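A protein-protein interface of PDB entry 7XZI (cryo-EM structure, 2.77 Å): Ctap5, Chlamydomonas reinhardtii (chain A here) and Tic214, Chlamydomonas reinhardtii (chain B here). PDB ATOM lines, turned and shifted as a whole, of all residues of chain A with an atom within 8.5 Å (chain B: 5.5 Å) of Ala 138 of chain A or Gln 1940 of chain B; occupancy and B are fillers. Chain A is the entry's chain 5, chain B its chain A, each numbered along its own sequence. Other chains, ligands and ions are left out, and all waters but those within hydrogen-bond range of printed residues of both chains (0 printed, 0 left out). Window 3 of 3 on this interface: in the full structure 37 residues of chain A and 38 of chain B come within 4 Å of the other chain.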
ATOM      1  N   ASP A 132     -17.825 -14.329  37.828  1.00  0.00           N
ATOM      2  CA  ASP A 132     -17.852 -13.598  36.564  1.00  0.00           C
ATOM      3  C   ASP A 132     -17.447 -14.490  35.398  1.00  0.00           C
ATOM      4  O   ASP A 132     -18.044 -14.416  34.317  1.00  0.00           O
ATOM      5  CB  ASP A 132     -16.939 -12.375  36.647  1.00  0.00           C
ATOM      6  N   GLU A 133     -16.430 -15.333  35.593  1.00  0.00           N
ATOM      7  CA  GLU A 133     -15.980 -16.213  34.521  1.00  0.00           C
ATOM      8  C   GLU A 133     -17.066 -17.207  34.124  1.00  0.00           C
ATOM      9  O   GLU A 133     -17.258 -17.487  32.935  1.00  0.00           O
ATOM     10  CB  GLU A 133     -14.708 -16.948  34.945  1.00  0.00           C
ATOM     11  N   GLU A 134     -17.783 -17.755  35.109  1.00  0.00           N
ATOM     12  CA  GLU A 134     -18.850 -18.705  34.809  1.00  0.00           C
ATOM     13  C   GLU A 134     -19.977 -18.042  34.026  1.00  0.00           C
ATOM     14  O   GLU A 134     -20.525 -18.633  33.089  1.00  0.00           O
ATOM     15  CB  GLU A 134     -19.382 -19.320  36.103  1.00  0.00           C
ATOM     16  N   ALA A 135     -20.340 -16.811  34.397  1.00  0.00           N
ATOM     17  CA  ALA A 135     -21.396 -16.103  33.687  1.00  0.00           C
ATOM     18  C   ALA A 135     -20.940 -15.590  32.329  1.00  0.00           C
ATOM     19  O   ALA A 135     -21.784 -15.323  31.466  1.00  0.00           O
ATOM     20  CB  ALA A 135     -21.911 -14.937  34.535  1.00  0.00           C
ATOM     21  N   GLU A 136     -19.629 -15.447  32.117  1.00  0.00           N
ATOM     22  CA  GLU A 136     -19.129 -14.982  30.829  1.00  0.00           C
ATOM     23  C   GLU A 136     -19.290 -16.025  29.731  1.00  0.00           C
ATOM     24  O   GLU A 136     -19.182 -15.682  28.549  1.00  0.00           O
ATOM     25  CB  GLU A 136     -17.658 -14.580  30.951  1.00  0.00           C
ATOM     26  N   ASP A 137     -19.544 -17.283  30.090  1.00  0.00           N
ATOM     27  CA  ASP A 137     -19.698 -18.365  29.125  1.00  0.00           C
ATOM     28  C   ASP A 137     -21.152 -18.808  28.992  1.00  0.00           C
ATOM     29  O   ASP A 137     -21.428 -19.943  28.599  1.00  0.00           O
ATOM     30  CB  ASP A 137     -18.813 -19.549  29.506  1.00  0.00           C
ATOM     31  N   ALA A 138     -22.091 -17.921  29.318  1.00  0.00           N
ATOM     32  CA  ALA A 138     -23.514 -18.220  29.212  1.00  0.00           C
ATOM     33  C   ALA A 138     -24.147 -17.689  27.935  1.00  0.00           C
ATOM     34  O   ALA A 138     -25.141 -18.255  27.469  1.00  0.00           O
ATOM     35  CB  ALA A 138     -24.267 -17.654  30.420  1.00  0.00           C
ATOM     36  N   THR A 139     -23.602 -16.617  27.362  1.00  0.00           N
ATOM     37  CA  THR A 139     -24.104 -16.050  26.120  1.00  0.00           C
ATOM     38  C   THR A 139     -22.940 -15.815  25.166  1.00  0.00           C
ATOM     39  O   THR A 139     -21.796 -15.621  25.584  1.00  0.00           O
ATOM     40  CB  THR A 139     -24.857 -14.732  26.357  1.00  0.00           C
ATOM     41  OG1 THR A 139     -24.010 -13.816  27.063  1.00  0.00           O
ATOM     42  CG2 THR A 139     -26.124 -14.973  27.167  1.00  0.00           C
ATOM     43  N   SER A 140     -23.247 -15.838  23.871  1.00  0.00           N
ATOM     44  CA  SER A 140     -22.242 -15.642  22.837  1.00  0.00           C
ATOM     45  C   SER A 140     -22.845 -14.844  21.690  1.00  0.00           C
ATOM     46  O   SER A 140     -24.065 -14.792  21.515  1.00  0.00           O
ATOM     47  CB  SER A 140     -21.690 -16.980  22.324  1.00  0.00           C
ATOM     48  OG  SER A 140     -22.723 -17.784  21.782  1.00  0.00           O
ATOM     49  N   LYS A 141     -21.971 -14.213  20.913  1.00  0.00           N
ATOM     50  CA  LYS A 141     -22.403 -13.425  19.770  1.00  0.00           C
ATOM     51  C   LYS A 141     -22.727 -14.331  18.584  1.00  0.00           C
ATOM     52  O   LYS A 141     -22.341 -15.501  18.536  1.00  0.00           O
ATOM     53  CB  LYS A 141     -21.332 -12.400  19.394  1.00  0.00           C
ATOM     54  CG  LYS A 141     -21.226 -11.243  20.380  1.00  0.00           C
ATOM     55  CD  LYS A 141     -20.057 -10.326  20.062  1.00  0.00           C
ATOM     56  CE  LYS A 141     -18.739 -10.913  20.538  1.00  0.00           C
ATOM     57  NZ  LYS A 141     -18.691 -11.045  22.019  1.00  0.00           N
ATOM     58  N   TYR A 149     -20.884 -23.574  16.477  1.00  0.00           N
ATOM     59  CA  TYR A 149     -21.947 -24.573  16.523  1.00  0.00           C
ATOM     60  C   TYR A 149     -22.539 -24.844  15.144  1.00  0.00           C
ATOM     61  O   TYR A 149     -22.928 -25.980  14.845  1.00  0.00           O
ATOM     62  CB  TYR A 149     -23.040 -24.124  17.493  1.00  0.00           C
ATOM     63  CG  TYR A 149     -22.668 -24.284  18.948  1.00  0.00           C
ATOM     64  CD1 TYR A 149     -22.880 -25.486  19.607  1.00  0.00           C
ATOM     65  CD2 TYR A 149     -22.109 -23.234  19.664  1.00  0.00           C
ATOM     66  CE1 TYR A 149     -22.546 -25.641  20.937  1.00  0.00           C
ATOM     67  CE2 TYR A 149     -21.770 -23.379  20.998  1.00  0.00           C
ATOM     68  CZ  TYR A 149     -21.991 -24.585  21.628  1.00  0.00           C
ATOM     69  OH  TYR A 149     -21.657 -24.737  22.954  1.00  0.00           O
ATOM     70  N   VAL B1923     -26.959 -13.810  21.499  1.00  0.00           N
ATOM     71  CA  VAL B1923     -27.900 -14.922  21.492  1.00  0.00           C
ATOM     72  C   VAL B1923     -27.539 -15.853  22.641  1.00  0.00           C
ATOM     73  O   VAL B1923     -26.359 -16.119  22.890  1.00  0.00           O
ATOM     74  CB  VAL B1923     -27.897 -15.670  20.141  1.00  0.00           C
ATOM     75  CG1 VAL B1923     -26.489 -16.096  19.758  1.00  0.00           C
ATOM     76  CG2 VAL B1923     -28.839 -16.868  20.182  1.00  0.00           C
ATOM     77  N   GLU B1924     -28.558 -16.333  23.351  1.00  0.00           N
ATOM     78  CA  GLU B1924     -28.357 -17.114  24.572  1.00  0.00           C
ATOM     79  C   GLU B1924     -28.089 -18.563  24.185  1.00  0.00           C
ATOM     80  O   GLU B1924     -29.008 -19.353  23.966  1.00  0.00           O
ATOM     81  CB  GLU B1924     -29.564 -16.986  25.493  1.00  0.00           C
ATOM     82  CG  GLU B1924     -29.287 -17.370  26.937  1.00  0.00           C
ATOM     83  CD  GLU B1924     -30.420 -16.980  27.867  1.00  0.00           C
ATOM     84  OE1 GLU B1924     -31.506 -16.627  27.362  1.00  0.00           O
ATOM     85  OE2 GLU B1924     -30.223 -17.022  29.100  1.00  0.00           O
ATOM     86  N   MET B1925     -26.805 -18.913  24.103  1.00  0.00           N
ATOM     87  CA  MET B1925     -26.369 -20.267  23.823  1.00  0.00           C
ATOM     88  C   MET B1925     -25.012 -20.435  24.495  1.00  0.00           C
ATOM     89  O   MET B1925     -24.126 -19.590  24.289  1.00  0.00           O
ATOM     90  CB  MET B1925     -26.264 -20.562  22.326  1.00  0.00           C
ATOM     91  CG  MET B1925     -25.912 -22.005  21.998  1.00  0.00           C
ATOM     92  SD  MET B1925     -26.149 -22.420  20.260  1.00  0.00           S
ATOM     93  CE  MET B1925     -27.933 -22.337  20.132  1.00  0.00           C
ATOM     94  N   PRO B1926     -24.825 -21.483  25.296  1.00  0.00           N
ATOM     95  CA  PRO B1926     -23.590 -21.604  26.080  1.00  0.00           C
ATOM     96  C   PRO B1926     -22.364 -21.786  25.197  1.00  0.00           C
ATOM     97  O   PRO B1926     -22.436 -22.353  24.105  1.00  0.00           O
ATOM     98  CB  PRO B1926     -23.842 -22.843  26.948  1.00  0.00           C
ATOM     99  CG  PRO B1926     -25.324 -23.029  26.943  1.00  0.00           C
ATOM    100  CD  PRO B1926     -25.785 -22.556  25.603  1.00  0.00           C
ATOM    101  N   LYS B1927     -21.232 -21.292  25.687  1.00  0.00           N
ATOM    102  CA  LYS B1927     -19.938 -21.499  25.055  1.00  0.00           C
ATOM    103  C   LYS B1927     -19.130 -22.497  25.875  1.00  0.00           C
ATOM    104  O   LYS B1927     -19.145 -22.458  27.108  1.00  0.00           O
ATOM    105  CB  LYS B1927     -19.172 -20.181  24.925  1.00  0.00           C
ATOM    106  N   LEU B1938     -23.761 -26.402  33.081  1.00  0.00           N
ATOM    107  CA  LEU B1938     -23.629 -25.241  32.211  1.00  0.00           C
ATOM    108  C   LEU B1938     -24.628 -24.137  32.532  1.00  0.00           C
ATOM    109  O   LEU B1938     -24.545 -23.062  31.928  1.00  0.00           O
ATOM    110  CB  LEU B1938     -23.790 -25.663  30.747  1.00  0.00           C
ATOM    111  CG  LEU B1938     -22.894 -26.808  30.270  1.00  0.00           C
ATOM    112  CD1 LEU B1938     -23.146 -27.112  28.801  1.00  0.00           C
ATOM    113  CD2 LEU B1938     -21.430 -26.481  30.513  1.00  0.00           C
ATOM    114  N   LYS B1939     -25.583 -24.392  33.432  1.00  0.00           N
ATOM    115  CA  LYS B1939     -26.634 -23.449  33.808  1.00  0.00           C
ATOM    116  C   LYS B1939     -27.572 -23.173  32.638  1.00  0.00           C
ATOM    117  O   LYS B1939     -28.507 -22.376  32.760  1.00  0.00           O
ATOM    118  CB  LYS B1939     -26.036 -22.140  34.343  1.00  0.00           C
ATOM    119  N   GLN B1940     -27.325 -23.824  31.498  1.00  0.00           N
ATOM    120  CA  GLN B1940     -28.196 -23.720  30.328  1.00  0.00           C
ATOM    121  C   GLN B1940     -27.927 -24.937  29.449  1.00  0.00           C
ATOM    122  O   GLN B1940     -26.855 -25.043  28.846  1.00  0.00           O
ATOM    123  CB  GLN B1940     -27.959 -22.421  29.571  1.00  0.00           C
ATOM    124  CG  GLN B1940     -28.822 -22.272  28.329  1.00  0.00           C
ATOM    125  CD  GLN B1940     -28.567 -20.978  27.588  1.00  0.00           C
ATOM    126  OE1 GLN B1940     -29.262 -20.656  26.623  1.00  0.00           O
ATOM    127  NE2 GLN B1940     -27.568 -20.227  28.034  1.00  0.00           N
ATOM    128  N   LYS B1941     -28.897 -25.848  29.385  1.00  0.00           N
ATOM    129  CA  LYS B1941     -28.753 -27.045  28.567  1.00  0.00           C
ATOM    130  C   LYS B1941     -28.615 -26.681  27.094  1.00  0.00           C
ATOM    131  O   LYS B1941     -29.269 -25.760  26.599  1.00  0.00           O
ATOM    132  CB  LYS B1941     -29.954 -27.971  28.773  1.00  0.00           C
ATOM    133  N   ILE B1942     -27.745 -27.415  26.391  1.00  0.00           N
ATOM    134  CA  ILE B1942     -27.532 -27.189  24.964  1.00  0.00           C
ATOM    135  C   ILE B1942     -28.685 -27.697  24.108  1.00  0.00           C
ATOM    136  O   ILE B1942     -28.632 -27.571  22.878  1.00  0.00           O
ATOM    137  CB  ILE B1942     -26.206 -27.838  24.511  1.00  0.00           C
ATOM    138  CG1 ILE B1942     -25.187 -27.850  25.652  1.00  0.00           C
ATOM    139  CG2 ILE B1942     -25.608 -27.082  23.331  1.00  0.00           C
ATOM    140  CD1 ILE B1942     -23.822 -28.389  25.249  1.00  0.00           C
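The backbone carbonyl oxygen (O) of Asp 137 of chain A sits at hydrogen-bond distance from the backbone NH (N) of Lys 1927 of chain B. O of Ala 138 of chain A lies within hydrogen-bond range of NE2 of Gln 1940 of chain B (3.2 Å). O of Ser 140 of chain A is in hydrogen-bond range of N of Val 1923 of chain B (3.1 Å). OG of Ser 140 of chain A lies within hydrogen-bond range of O of Met 1925 of chain B (3.4 Å). OH of Tyr 149 of chain A is in hydrogen-bond range of O of Pro 1926 of chain B, at 2.8 Å.
Printed residues of chain A within 4 Å of Gln 1940 of chain B: Ala 138 (3.2 Å). No residue of chain A comes within 4 Å of Lys 1939 of chain B. No residue of chain A comes within 4 Å of Lys 1941 of chain B. Of the printed residues of chain A, Met 1925 of chain B touches Ala 138, Thr 139 and Ser 140. Of the printed residues of chain A, Val 1923 of chain B touches Thr 139 and Ser 140. Printed residues of chain B within 4 Å of Thr 139 of chain A: Val 1923 (3.9 Å), Glu 1924 (3.98 Å) and Met 1925 (3.99 Å). Glu 133 of chain A touches none of the printed residues of chain B.
Printed residues of chain A that touch a printed residue of chain B: Asp 137, Ala 138, Thr 139, Ser 140 and Tyr 149. Hydrophobic or aromatic side chains of chain A within 4 Å of the printed part of chain B: Tyr 149. Printed residues of chain B that touch a printed residue of chain A: Val 1923, Glu 1924, Met 1925, Pro 1926, Lys 1927 and Gln 1940. Hydrophobic or aromatic side chains of chain B that line the printed part of chain A: Val 1923. Among the printed residues, no Asp or Glu carboxylate lies within 4 Å of a Lys or Arg side-chain nitrogen of the other chain.
O of Glu 1924 of chain B sits close to OE1 of Gln 1940 of chain B (3.0 Å).
Among the printed residues, merely in contact across the chains: Ala 138 of chain A with Met 1925 of chain B, Asp 137 of chain A with Pro 1926 of chain B, Ala 138 of chain A with Pro 1926 of chain B, Thr 139 of chain A with Val 1923 of chain B, Thr 139 of chain A with Glu 1924 of chain B and Thr 139 of chain A with Met 1925 of chain B.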
